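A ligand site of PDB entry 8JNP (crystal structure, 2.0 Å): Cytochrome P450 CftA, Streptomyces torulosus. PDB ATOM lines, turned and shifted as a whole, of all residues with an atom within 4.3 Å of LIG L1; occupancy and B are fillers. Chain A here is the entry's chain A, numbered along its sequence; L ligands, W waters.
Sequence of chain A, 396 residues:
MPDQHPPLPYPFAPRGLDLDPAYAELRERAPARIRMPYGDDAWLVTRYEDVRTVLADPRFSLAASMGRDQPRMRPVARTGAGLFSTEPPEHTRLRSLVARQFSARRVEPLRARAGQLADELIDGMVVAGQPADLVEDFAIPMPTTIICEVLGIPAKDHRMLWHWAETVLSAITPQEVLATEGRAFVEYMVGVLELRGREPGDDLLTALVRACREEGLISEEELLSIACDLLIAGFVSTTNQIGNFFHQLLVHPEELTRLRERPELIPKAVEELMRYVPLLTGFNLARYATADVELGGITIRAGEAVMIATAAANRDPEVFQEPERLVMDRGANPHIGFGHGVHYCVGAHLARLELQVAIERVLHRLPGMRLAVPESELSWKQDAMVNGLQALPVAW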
ATOM      1  N   LEU A  55      -1.813  42.598  23.062  1.00  0.00           N
ATOM      2  CA  LEU A  55      -1.290  41.522  23.916  1.00  0.00           C
ATOM      3  C   LEU A  55      -0.565  42.043  25.160  1.00  0.00           C
ATOM      4  O   LEU A  55      -0.486  41.309  26.166  1.00  0.00           O
ATOM      5  CB  LEU A  55      -0.374  40.627  23.074  1.00  0.00           C
ATOM      6  CG  LEU A  55      -1.022  39.815  21.952  1.00  0.00           C
ATOM      7  CD1 LEU A  55       0.080  39.074  21.101  1.00  0.00           C
ATOM      8  CD2 LEU A  55      -1.998  38.873  22.568  1.00  0.00           C
ATOM      9  N   LEU A  83      -6.067  29.564  32.793  1.00  0.00           N
ATOM     10  CA  LEU A  83      -5.129  30.490  32.182  1.00  0.00           C
ATOM     11  C   LEU A  83      -5.790  31.369  31.116  1.00  0.00           C
ATOM     12  O   LEU A  83      -5.473  32.564  31.019  1.00  0.00           O
ATOM     13  CB  LEU A  83      -3.962  29.718  31.576  1.00  0.00           C
ATOM     14  CG  LEU A  83      -3.141  28.898  32.547  1.00  0.00           C
ATOM     15  CD1 LEU A  83      -2.175  27.961  31.827  1.00  0.00           C
ATOM     16  CD2 LEU A  83      -2.370  29.872  33.502  1.00  0.00           C
ATOM     17  N   PHE A  84      -6.694  30.799  30.318  1.00  0.00           N
ATOM     18  CA  PHE A  84      -7.368  31.572  29.266  1.00  0.00           C
ATOM     19  C   PHE A  84      -8.451  32.479  29.799  1.00  0.00           C
ATOM     20  O   PHE A  84      -9.092  33.183  29.001  1.00  0.00           O
ATOM     21  CB  PHE A  84      -8.030  30.646  28.217  1.00  0.00           C
ATOM     22  CG  PHE A  84      -7.104  29.642  27.626  1.00  0.00           C
ATOM     23  CD1 PHE A  84      -6.043  30.045  26.870  1.00  0.00           C
ATOM     24  CD2 PHE A  84      -7.319  28.282  27.814  1.00  0.00           C
ATOM     25  CE1 PHE A  84      -5.175  29.117  26.325  1.00  0.00           C
ATOM     26  CE2 PHE A  84      -6.431  27.366  27.271  1.00  0.00           C
ATOM     27  CZ  PHE A  84      -5.369  27.777  26.559  1.00  0.00           C
ATOM     28  N   HIS A  91      -3.941  35.023  37.323  1.00  0.00           N
ATOM     29  CA  HIS A  91      -3.272  34.287  36.266  1.00  0.00           C
ATOM     30  C   HIS A  91      -1.865  33.885  36.692  1.00  0.00           C
ATOM     31  O   HIS A  91      -1.388  32.779  36.372  1.00  0.00           O
ATOM     32  CB  HIS A  91      -3.194  35.136  34.997  1.00  0.00           C
ATOM     33  CG  HIS A  91      -2.434  34.484  33.885  1.00  0.00           C
ATOM     34  ND1 HIS A  91      -1.071  34.611  33.728  1.00  0.00           N
ATOM     35  CD2 HIS A  91      -2.862  33.696  32.863  1.00  0.00           C
ATOM     36  CE1 HIS A  91      -0.681  33.913  32.669  1.00  0.00           C
ATOM     37  NE2 HIS A  91      -1.748  33.366  32.121  1.00  0.00           N
ATOM     38  N   ARG A  95      -0.172  30.248  36.545  1.00  0.00           N
ATOM     39  CA  ARG A  95       0.911  30.002  35.602  1.00  0.00           C
ATOM     40  C   ARG A  95       2.218  29.619  36.301  1.00  0.00           C
ATOM     41  O   ARG A  95       2.961  28.771  35.795  1.00  0.00           O
ATOM     42  CB  ARG A  95       1.062  31.240  34.719  1.00  0.00           C
ATOM     43  CG  ARG A  95       2.292  31.196  33.850  1.00  0.00           C
ATOM     44  CD  ARG A  95       1.924  30.902  32.411  1.00  0.00           C
ATOM     45  NE  ARG A  95       3.101  30.942  31.542  1.00  0.00           N
ATOM     46  CZ  ARG A  95       3.059  31.303  30.270  1.00  0.00           C
ATOM     47  NH1 ARG A  95       1.919  31.646  29.693  1.00  0.00           N
ATOM     48  NH2 ARG A  95       4.187  31.333  29.575  1.00  0.00           N
ATOM     49  N   PHE A 102       7.162  23.378  32.098  1.00  0.00           N
ATOM     50  CA  PHE A 102       7.202  23.777  30.704  1.00  0.00           C
ATOM     51  C   PHE A 102       8.384  24.665  30.390  1.00  0.00           C
ATOM     52  O   PHE A 102       8.559  25.021  29.217  1.00  0.00           O
ATOM     53  CB  PHE A 102       5.872  24.437  30.312  1.00  0.00           C
ATOM     54  CG  PHE A 102       4.738  23.419  30.177  1.00  0.00           C
ATOM     55  CD1 PHE A 102       4.585  22.704  29.023  1.00  0.00           C
ATOM     56  CD2 PHE A 102       3.880  23.151  31.232  1.00  0.00           C
ATOM     57  CE1 PHE A 102       3.584  21.743  28.876  1.00  0.00           C
ATOM     58  CE2 PHE A 102       2.896  22.174  31.124  1.00  0.00           C
ATOM     59  CZ  PHE A 102       2.726  21.468  29.924  1.00  0.00           C
ATOM     60  N   ILE A 147       2.662  14.734  25.490  1.00  0.00           N
ATOM     61  CA  ILE A 147       1.946  15.528  26.477  1.00  0.00           C
ATOM     62  C   ILE A 147       1.284  14.597  27.510  1.00  0.00           C
ATOM     63  O   ILE A 147       1.205  14.928  28.691  1.00  0.00           O
ATOM     64  CB  ILE A 147       0.959  16.482  25.793  1.00  0.00           C
ATOM     65  CG1 ILE A 147       0.416  17.512  26.795  1.00  0.00           C
ATOM     66  CG2 ILE A 147      -0.219  15.705  25.164  1.00  0.00           C
ATOM     67  CD1 ILE A 147       1.487  18.297  27.535  1.00  0.00           C
ATOM     68  N   LEU A 230      -4.446  22.267  29.527  1.00  0.00           N
ATOM     69  CA  LEU A 230      -3.139  21.818  29.065  1.00  0.00           C
ATOM     70  C   LEU A 230      -3.243  20.588  28.148  1.00  0.00           C
ATOM     71  O   LEU A 230      -2.481  20.451  27.162  1.00  0.00           O
ATOM     72  CB  LEU A 230      -2.255  21.490  30.267  1.00  0.00           C
ATOM     73  CG  LEU A 230      -1.720  22.708  31.039  1.00  0.00           C
ATOM     74  CD1 LEU A 230      -0.805  22.307  32.181  1.00  0.00           C
ATOM     75  CD2 LEU A 230      -0.972  23.680  30.105  1.00  0.00           C
ATOM     76  N   ALA A 233      -4.984  21.714  24.636  1.00  0.00           N
ATOM     77  CA  ALA A 233      -4.020  22.492  23.858  1.00  0.00           C
ATOM     78  C   ALA A 233      -2.907  21.615  23.309  1.00  0.00           C
ATOM     79  O   ALA A 233      -2.513  21.744  22.147  1.00  0.00           O
ATOM     80  CB  ALA A 233      -3.443  23.613  24.722  1.00  0.00           C
ATOM     81  N   GLY A 234      -2.369  20.731  24.154  1.00  0.00           N
ATOM     82  CA  GLY A 234      -1.358  19.795  23.681  1.00  0.00           C
ATOM     83  C   GLY A 234      -1.839  18.837  22.599  1.00  0.00           C
ATOM     84  O   GLY A 234      -1.038  18.356  21.812  1.00  0.00           O
ATOM     85  N   SER A 237      -2.671  21.245  18.954  1.00  0.00           N
ATOM     86  CA  SER A 237      -1.747  22.237  18.381  1.00  0.00           C
ATOM     87  C   SER A 237      -0.693  21.547  17.519  1.00  0.00           C
ATOM     88  O   SER A 237      -0.732  21.604  16.296  1.00  0.00           O
ATOM     89  CB  SER A 237      -1.145  23.081  19.520  1.00  0.00           C
ATOM     90  OG  SER A 237      -0.466  22.279  20.464  1.00  0.00           O
ATOM     91  N   THR A 238       0.249  20.877  18.174  1.00  0.00           N
ATOM     92  CA  THR A 238       1.413  20.369  17.488  1.00  0.00           C
ATOM     93  C   THR A 238       1.090  19.231  16.530  1.00  0.00           C
ATOM     94  O   THR A 238       1.828  19.043  15.563  1.00  0.00           O
ATOM     95  CB  THR A 238       2.431  19.936  18.526  1.00  0.00           C
ATOM     96  OG1 THR A 238       2.513  20.949  19.513  1.00  0.00           O
ATOM     97  CG2 THR A 238       3.789  19.822  17.902  1.00  0.00           C
ATOM     98  N   GLN A 241       0.468  21.110  13.448  1.00  0.00           N
ATOM     99  CA  GLN A 241       1.602  21.902  13.010  1.00  0.00           C
ATOM    100  C   GLN A 241       2.712  21.036  12.426  1.00  0.00           C
ATOM    101  O   GLN A 241       3.416  21.466  11.514  1.00  0.00           O
ATOM    102  CB  GLN A 241       2.131  22.735  14.180  1.00  0.00           C
ATOM    103  CG  GLN A 241       3.112  23.848  13.775  1.00  0.00           C
ATOM    104  CD  GLN A 241       2.432  25.062  13.138  1.00  0.00           C
ATOM    105  OE1 GLN A 241       1.599  24.922  12.214  1.00  0.00           O
ATOM    106  NE2 GLN A 241       2.783  26.263  13.627  1.00  0.00           N
ATOM    107  N   MET A 274       7.155  28.763  12.004  1.00  0.00           N
ATOM    108  CA  MET A 274       6.256  29.321  13.016  1.00  0.00           C
ATOM    109  C   MET A 274       5.703  30.674  12.576  1.00  0.00           C
ATOM    110  O   MET A 274       4.506  30.976  12.769  1.00  0.00           O
ATOM    111  CB  MET A 274       6.974  29.496  14.346  1.00  0.00           C
ATOM    112  CG  MET A 274       7.138  28.289  15.260  1.00  0.00           C
ATOM    113  SD  MET A 274       5.566  27.425  15.691  1.00  0.00           S
ATOM    114  CE  MET A 274       4.727  28.749  16.592  1.00  0.00           C
ATOM    115  N   LEU A 279      -1.750  28.677  11.651  1.00  0.00           N
ATOM    116  CA  LEU A 279      -2.184  27.455  12.300  1.00  0.00           C
ATOM    117  C   LEU A 279      -3.584  27.632  12.875  1.00  0.00           C
ATOM    118  O   LEU A 279      -4.547  27.018  12.400  1.00  0.00           O
ATOM    119  CB  LEU A 279      -1.189  27.055  13.393  1.00  0.00           C
ATOM    120  CG  LEU A 279      -1.634  25.841  14.249  1.00  0.00           C
ATOM    121  CD1 LEU A 279      -1.757  24.644  13.333  1.00  0.00           C
ATOM    122  CD2 LEU A 279      -0.715  25.509  15.424  1.00  0.00           C
ATOM    123  N   LEU A 280      -3.712  28.476  13.884  1.00  0.00           N
ATOM    124  CA  LEU A 280      -4.952  28.590  14.641  1.00  0.00           C
ATOM    125  C   LEU A 280      -5.941  29.465  13.894  1.00  0.00           C
ATOM    126  O   LEU A 280      -5.616  30.598  13.544  1.00  0.00           O
ATOM    127  CB  LEU A 280      -4.663  29.187  16.027  1.00  0.00           C
ATOM    128  CG  LEU A 280      -3.602  28.453  16.870  1.00  0.00           C
ATOM    129  CD1 LEU A 280      -3.326  29.205  18.165  1.00  0.00           C
ATOM    130  CD2 LEU A 280      -4.109  27.023  17.204  1.00  0.00           C
ATOM    131  N   LEU A 285      -8.795  33.690  20.920  1.00  0.00           N
ATOM    132  CA  LEU A 285      -9.329  34.235  22.152  1.00  0.00           C
ATOM    133  C   LEU A 285      -9.778  35.660  21.891  1.00  0.00           C
ATOM    134  O   LEU A 285      -9.076  36.435  21.238  1.00  0.00           O
ATOM    135  CB  LEU A 285      -8.267  34.220  23.237  1.00  0.00           C
ATOM    136  CG  LEU A 285      -7.770  32.815  23.596  1.00  0.00           C
ATOM    137  CD1 LEU A 285      -6.541  32.879  24.488  1.00  0.00           C
ATOM    138  CD2 LEU A 285      -8.847  32.005  24.267  1.00  0.00           C
ATOM    139  N   ARG A 287     -10.468  39.223  23.669  1.00  0.00           N
ATOM    140  CA  ARG A 287     -10.333  40.038  24.873  1.00  0.00           C
ATOM    141  C   ARG A 287     -11.404  41.134  24.845  1.00  0.00           C
ATOM    142  O   ARG A 287     -11.872  41.535  23.785  1.00  0.00           O
ATOM    143  CB  ARG A 287      -8.936  40.644  24.948  1.00  0.00           C
ATOM    144  CG  ARG A 287      -7.870  39.544  25.127  1.00  0.00           C
ATOM    145  CD  ARG A 287      -6.495  39.920  24.622  1.00  0.00           C
ATOM    146  NE  ARG A 287      -5.455  39.002  25.095  1.00  0.00           N
ATOM    147  CZ  ARG A 287      -5.068  37.902  24.463  1.00  0.00           C
ATOM    148  NH1 ARG A 287      -5.691  37.469  23.369  1.00  0.00           N
ATOM    149  NH2 ARG A 287      -4.045  37.198  24.940  1.00  0.00           N
ATOM    150  N   ILE A 308      -7.290  39.275  17.482  1.00  0.00           N
ATOM    151  CA  ILE A 308      -6.016  39.499  16.815  1.00  0.00           C
ATOM    152  C   ILE A 308      -5.874  38.443  15.722  1.00  0.00           C
ATOM    153  O   ILE A 308      -6.499  37.381  15.765  1.00  0.00           O
ATOM    154  CB  ILE A 308      -4.844  39.431  17.801  1.00  0.00           C
ATOM    155  CG1 ILE A 308      -4.700  38.010  18.358  1.00  0.00           C
ATOM    156  CG2 ILE A 308      -4.990  40.449  18.953  1.00  0.00           C
ATOM    157  CD1 ILE A 308      -3.434  37.864  19.241  1.00  0.00           C
ATOM    158  N   GLY A 337       4.012  34.007  16.572  1.00  0.00           N
ATOM    159  CA  GLY A 337       3.358  32.721  16.388  1.00  0.00           C
ATOM    160  C   GLY A 337       3.016  32.031  17.694  1.00  0.00           C
ATOM    161  O   GLY A 337       2.230  31.082  17.686  1.00  0.00           O
ATOM    162  N   PHE A 338       3.673  32.413  18.788  1.00  0.00           N
ATOM    163  CA  PHE A 338       3.334  31.924  20.120  1.00  0.00           C
ATOM    164  C   PHE A 338       2.734  33.001  21.010  1.00  0.00           C
ATOM    165  O   PHE A 338       2.730  32.848  22.227  1.00  0.00           O
ATOM    166  CB  PHE A 338       4.556  31.360  20.852  1.00  0.00           C
ATOM    167  CG  PHE A 338       5.034  30.014  20.354  1.00  0.00           C
ATOM    168  CD1 PHE A 338       4.223  28.872  20.395  1.00  0.00           C
ATOM    169  CD2 PHE A 338       6.332  29.892  19.876  1.00  0.00           C
ATOM    170  CE1 PHE A 338       4.710  27.632  19.938  1.00  0.00           C
ATOM    171  CE2 PHE A 338       6.826  28.674  19.425  1.00  0.00           C
ATOM    172  CZ  PHE A 338       6.015  27.519  19.451  1.00  0.00           C
ATOM    173  N   GLY A 339       2.279  34.098  20.448  1.00  0.00           N
ATOM    174  CA  GLY A 339       1.719  35.140  21.269  1.00  0.00           C
ATOM    175  C   GLY A 339       2.784  36.059  21.855  1.00  0.00           C
ATOM    176  O   GLY A 339       3.917  36.129  21.376  1.00  0.00           O
ATOM    177  N   VAL A 342       1.470  38.375  28.854  1.00  0.00           N
ATOM    178  CA  VAL A 342       1.283  37.417  29.937  1.00  0.00           C
ATOM    179  C   VAL A 342       0.713  36.092  29.447  1.00  0.00           C
ATOM    180  O   VAL A 342       0.950  35.045  30.069  1.00  0.00           O
ATOM    181  CB  VAL A 342       0.414  37.992  31.089  1.00  0.00           C
ATOM    182  CG1 VAL A 342       0.635  39.527  31.320  1.00  0.00           C
ATOM    183  CG2 VAL A 342      -1.036  37.650  30.911  1.00  0.00           C
ATOM    184  N   HIS A 343      -0.062  36.058  28.345  1.00  0.00           N
ATOM    185  CA  HIS A 343      -0.552  34.756  27.852  1.00  0.00           C
ATOM    186  C   HIS A 343       0.366  34.137  26.786  1.00  0.00           C
ATOM    187  O   HIS A 343      -0.064  33.217  26.063  1.00  0.00           O
ATOM    188  CB  HIS A 343      -1.994  34.891  27.355  1.00  0.00           C
ATOM    189  CG  HIS A 343      -2.925  35.405  28.435  1.00  0.00           C
ATOM    190  ND1 HIS A 343      -3.462  34.574  29.395  1.00  0.00           N
ATOM    191  CD2 HIS A 343      -3.280  36.657  28.774  1.00  0.00           C
ATOM    192  CE1 HIS A 343      -4.146  35.302  30.263  1.00  0.00           C
ATOM    193  NE2 HIS A 343      -4.061  36.570  29.904  1.00  0.00           N
ATOM    194  N   TYR A 344       1.613  34.597  26.687  1.00  0.00           N
ATOM    195  CA  TYR A 344       2.614  33.953  25.830  1.00  0.00           C
ATOM    196  C   TYR A 344       2.618  32.431  26.040  1.00  0.00           C
ATOM    197  O   TYR A 344       2.593  31.936  27.170  1.00  0.00           O
ATOM    198  CB  TYR A 344       4.006  34.547  26.116  1.00  0.00           C
ATOM    199  CG  TYR A 344       5.121  33.909  25.281  1.00  0.00           C
ATOM    200  CD1 TYR A 344       5.340  34.298  23.969  1.00  0.00           C
ATOM    201  CD2 TYR A 344       5.888  32.850  25.801  1.00  0.00           C
ATOM    202  CE1 TYR A 344       6.337  33.687  23.191  1.00  0.00           C
ATOM    203  CE2 TYR A 344       6.854  32.247  25.033  1.00  0.00           C
ATOM    204  CZ  TYR A 344       7.064  32.671  23.718  1.00  0.00           C
ATOM    205  OH  TYR A 344       8.031  32.115  22.923  1.00  0.00           O
ATOM    206  N   CYS A 345       2.669  31.692  24.936  1.00  0.00           N
ATOM    207  CA  CYS A 345       2.328  30.263  24.946  1.00  0.00           C
ATOM    208  C   CYS A 345       3.129  29.501  26.000  1.00  0.00           C
ATOM    209  O   CYS A 345       4.365  29.438  25.943  1.00  0.00           O
ATOM    210  CB  CYS A 345       2.534  29.657  23.550  1.00  0.00           C
ATOM    211  SG  CYS A 345       2.350  27.869  23.547  1.00  0.00           S
ATOM    212  N   VAL A 346       2.452  28.916  26.977  1.00  0.00           N
ATOM    213  CA  VAL A 346       3.187  28.160  27.995  1.00  0.00           C
ATOM    214  C   VAL A 346       3.790  26.887  27.407  1.00  0.00           C
ATOM    215  O   VAL A 346       4.721  26.311  27.996  1.00  0.00           O
ATOM    216  CB  VAL A 346       2.264  27.841  29.181  1.00  0.00           C
ATOM    217  CG1 VAL A 346       1.244  26.769  28.788  1.00  0.00           C
ATOM    218  CG2 VAL A 346       3.089  27.439  30.413  1.00  0.00           C
ATOM    219  N   GLY A 347       3.284  26.447  26.267  1.00  0.00           N
ATOM    220  CA  GLY A 347       3.819  25.278  25.610  1.00  0.00           C
ATOM    221  C   GLY A 347       4.929  25.540  24.598  1.00  0.00           C
ATOM    222  O   GLY A 347       5.335  24.596  23.908  1.00  0.00           O
ATOM    223  N   ALA A 351       6.599  22.660  22.360  1.00  0.00           N
ATOM    224  CA  ALA A 351       6.241  22.626  20.947  1.00  0.00           C
ATOM    225  C   ALA A 351       7.466  22.758  20.060  1.00  0.00           C
ATOM    226  O   ALA A 351       7.617  22.056  19.059  1.00  0.00           O
ATOM    227  CB  ALA A 351       5.220  23.730  20.642  1.00  0.00           C
ATOM    228  N   LEU A 355       8.727  20.082  17.269  1.00  0.00           N
ATOM    229  CA  LEU A 355       8.856  20.407  15.863  1.00  0.00           C
ATOM    230  C   LEU A 355      10.287  20.157  15.400  1.00  0.00           C
ATOM    231  O   LEU A 355      10.503  19.616  14.319  1.00  0.00           O
ATOM    232  CB  LEU A 355       8.442  21.861  15.599  1.00  0.00           C
ATOM    233  CG  LEU A 355       6.970  22.118  15.874  1.00  0.00           C
ATOM    234  CD1 LEU A 355       6.605  23.587  15.975  1.00  0.00           C
ATOM    235  CD2 LEU A 355       6.013  21.421  14.847  1.00  0.00           C
HETATM  236  C1  LIG L   1      -1.256  30.319  24.361  1.00  0.00           C
HETATM  237  C2  LIG L   1       0.075  29.162  19.871  1.00  0.00           C
HETATM  238  C3  LIG L   1       1.273  24.722  21.345  1.00  0.00           C
HETATM  239  C4  LIG L   1      -0.840  25.648  25.605  1.00  0.00           C
HETATM  240  C5  LIG L   1      -0.945  30.401  23.038  1.00  0.00           C
HETATM  241  C6  LIG L   1      -1.046  31.565  22.220  1.00  0.00           C
HETATM  242  C7  LIG L   1      -0.673  31.241  20.987  1.00  0.00           C
HETATM  243  C8  LIG L   1      -0.339  29.849  20.982  1.00  0.00           C
HETATM  244  C9  LIG L   1      -0.653  32.201  19.788  1.00  0.00           C
HETATM  245  C10 LIG L   1      -1.473  32.996  22.638  1.00  0.00           C
HETATM  246  C11 LIG L   1      -2.930  33.251  22.318  1.00  0.00           C
HETATM  247  C12 LIG L   1      -3.407  34.642  22.751  1.00  0.00           C
HETATM  248  O1  LIG L   1      -4.479  35.063  22.245  1.00  0.00           O
HETATM  249  O2  LIG L   1      -2.743  35.308  23.613  1.00  0.00           O
HETATM  250  C13 LIG L   1       0.549  27.880  19.848  1.00  0.00           C
HETATM  251  C14 LIG L   1       1.095  27.174  18.700  1.00  0.00           C
HETATM  252  C15 LIG L   1       1.400  25.922  19.146  1.00  0.00           C
HETATM  253  C16 LIG L   1       1.066  25.825  20.551  1.00  0.00           C
HETATM  254  C17 LIG L   1       1.233  27.780  17.263  1.00  0.00           C
HETATM  255  C18 LIG L   1       2.031  24.726  18.397  1.00  0.00           C
HETATM  256  C19 LIG L   1       2.918  24.901  17.431  1.00  0.00           C
HETATM  257  C20 LIG L   1       0.862  24.592  22.654  1.00  0.00           C
HETATM  258  C21 LIG L   1       1.129  23.453  23.538  1.00  0.00           C
HETATM  259  C22 LIG L   1       0.533  23.725  24.708  1.00  0.00           C
HETATM  260  C23 LIG L   1      -0.097  25.036  24.605  1.00  0.00           C
HETATM  261  C24 LIG L   1       1.947  22.194  23.125  1.00  0.00           C
HETATM  262  C25 LIG L   1       0.449  22.939  26.042  1.00  0.00           C
HETATM  263  C26 LIG L   1       1.166  21.854  26.286  1.00  0.00           C
HETATM  264  C27 LIG L   1      -1.145  26.986  25.626  1.00  0.00           C
HETATM  265  C28 LIG L   1      -1.713  27.662  26.751  1.00  0.00           C
HETATM  266  C29 LIG L   1      -1.808  28.969  26.432  1.00  0.00           C
HETATM  267  C30 LIG L   1      -1.315  29.136  25.067  1.00  0.00           C
HETATM  268  C31 LIG L   1      -2.156  26.958  28.068  1.00  0.00           C
HETATM  269  C32 LIG L   1      -2.381  30.082  27.299  1.00  0.00           C
HETATM  270  C33 LIG L   1      -1.283  30.531  28.272  1.00  0.00           C
HETATM  271  C34 LIG L   1      -1.734  31.574  29.266  1.00  0.00           C
HETATM  272  O3  LIG L   1      -2.802  32.190  29.121  1.00  0.00           O
HETATM  273  O4  LIG L   1      -0.975  31.836  30.252  1.00  0.00           O
HETATM  274  N1  LIG L   1      -0.518  29.341  22.259  1.00  0.00           N
HETATM  275  N2  LIG L   1       0.539  27.038  20.931  1.00  0.00           N
HETATM  276  N3  LIG L   1       0.129  25.551  23.342  1.00  0.00           N
HETATM  277  N4  LIG L   1      -0.912  27.910  24.594  1.00  0.00           N
HETATM  278 FE1  LIG L   1       0.179  27.513  22.892  1.00  0.00          FE
HETATM  279  C1  LG2 L   2      -9.143  27.822  23.888  1.00  0.00           C
HETATM  280  C2  LG2 L   2      -3.392  27.222  21.612  1.00  0.00           C
HETATM  281  C3  LG2 L   2     -10.523  24.325  23.066  1.00  0.00           C
HETATM  282  C4  LG2 L   2     -12.470  23.589  24.540  1.00  0.00           C
HETATM  283  C5  LG2 L   2     -11.209  24.025  24.368  1.00  0.00           C
HETATM  284  C6  LG2 L   2     -16.434  23.477  25.335  1.00  0.00           C
HETATM  285  C7  LG2 L   2     -12.743  27.119  23.825  1.00  0.00           C
HETATM  286  C8  LG2 L   2      -9.723  25.644  22.994  1.00  0.00           C
HETATM  287  C9  LG2 L   2     -11.538  27.401  23.394  1.00  0.00           C
HETATM  288  C10 LG2 L   2     -13.471  23.375  23.474  1.00  0.00           C
HETATM  289  C11 LG2 L   2     -15.358  22.433  25.013  1.00  0.00           C
HETATM  290  C12 LG2 L   2     -16.853  24.454  24.224  1.00  0.00           C
HETATM  291  C13 LG2 L   2     -13.983  27.705  23.355  1.00  0.00           C
HETATM  292  C14 LG2 L   2     -16.522  27.671  23.140  1.00  0.00           C
HETATM  293  C15 LG2 L   2     -15.196  27.293  23.766  1.00  0.00           C
HETATM  294  C16 LG2 L   2     -16.910  25.919  24.678  1.00  0.00           C
HETATM  295  N1  LG2 L   2     -14.729  22.787  23.711  1.00  0.00           N
HETATM  296  C17 LG2 L   2      -4.902  27.408  21.410  1.00  0.00           C
HETATM  297  C18 LG2 L   2     -10.266  26.780  23.904  1.00  0.00           C
HETATM  298  C19 LG2 L   2      -2.843  25.988  20.918  1.00  0.00           C
HETATM  299  C20 LG2 L   2      -4.401  29.963  21.606  1.00  0.00           C
HETATM  300  C21 LG2 L   2      -5.438  28.851  21.500  1.00  0.00           C
HETATM  301  C22 LG2 L   2      -6.432  28.854  22.669  1.00  0.00           C
HETATM  302  C23 LG2 L   2     -15.454  26.378  24.860  1.00  0.00           C
HETATM  303  C24 LG2 L   2      -7.024  27.486  22.549  1.00  0.00           C
HETATM  304  C25 LG2 L   2      -5.745  26.654  22.485  1.00  0.00           C
HETATM  305  C26 LG2 L   2      -7.862  27.015  23.750  1.00  0.00           C
HETATM  306  C27 LG2 L   2      -8.278  25.538  23.558  1.00  0.00           C
HETATM  307  C28 LG2 L   2      -7.237  24.733  22.836  1.00  0.00           C
HETATM  308  C29 LG2 L   2      -6.081  25.200  22.357  1.00  0.00           C
HETATM  309  N2  LG2 L   2     -17.429  26.812  23.663  1.00  0.00           N
HETATM  310  O1  LG2 L   2     -13.351  23.804  22.323  1.00  0.00           O
HETATM  311  O2  LG2 L   2     -13.864  28.692  22.453  1.00  0.00           O
HETATM  312  O3  LG2 L   2     -16.776  28.615  22.383  1.00  0.00           O
HETATM  313  O4  LG2 L   2     -14.715  25.990  25.733  1.00  0.00           O
HETATM  314  O   HOH W   1      -0.153  35.825  23.882  1.00  0.00           O
HETATM  315  O   HOH W   2      -5.871  33.985  20.483  1.00  0.00           O
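ND1 of His 343 sits at hydrogen-bond distance from O3 of LIG L1 (2.5 Å). FE1 of LIG L1 is bound by SG of Cys 345 (2.3 Å). O2 of LIG L1 lies within salt-bridge range of NH2 of Arg 287 (2.7 Å). NE2 of His 91 is in hydrogen-bond range of O4 of LIG L1, at 2.5 Å. An oxygen (O4) of LIG L1 lies within salt-bridge range of the guanidinium group of Arg 95 (3.0 Å).
The backbone NH (N) of Cys 345 lies within hydrogen-bond range of the backbone carbonyl oxygen (O) of Phe 338 (2.9 Å). ND1 of His 343 sits close to O of Leu 83, 3.3 Å away. N of Gly 347 lies close to SG of Cys 345 (3.2 Å). ND1 of His 343 is in hydrogen-bond range of NE2 of His 91, 3.4 Å away. SD of Met 274 lies within hydrogen-bond range of NE2 of Gln 241, 3.7 Å away. OG1 of Thr 238 is in hydrogen-bond range of OG of Ser 237, at 3.4 Å. The side-chain hydroxyl (OG) of Ser 237 lies within hydrogen-bond range of the backbone carbonyl oxygen (O) of Ala 233, 2.7 Å away. The guanidinium group (NH1) of Arg 95 is in hydrogen-bond range of the backbone carbonyl oxygen (O) of Tyr 344.
The backbone carbonyl oxygen (O) of Leu 83 lies close to an oxygen (O3) of LIG L1 (3.3 Å). Residues that only touch LIG L1: Phe 84 (3.1 Å), Ser 237 (3.1 Å), Ala 233 (3.4 Å), Gly 337 (3.5 Å), Val 346 (3.5 Å), Leu 279 (3.5 Å), Phe 102 (3.5 Å), Gly 339 (3.6 Å), Met 274 (3.7 Å), Phe 338 (3.7 Å), Gly 347 (3.7 Å), Val 342 (3.7 Å), Leu 285 (3.7 Å), Ile 147 (3.8 Å), Leu 55 (3.8 Å), Leu 280 (3.8 Å), Gln 241 (3.8 Å) and Thr 238 (3.9 Å). Along chain A the residues within 4 Å of LIG L1 span positions 55 to 347. The nearest printed residue that does not touch LIG L1 is Leu 230 (4.004 Å).
Water W2 lies within hydrogen-bond range of O1 of LIG L1 (2.5 Å) and N of Leu 285 (3.0 Å). Water W1 lies within hydrogen-bond range of O2 of LIG L1 and O of His 343.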
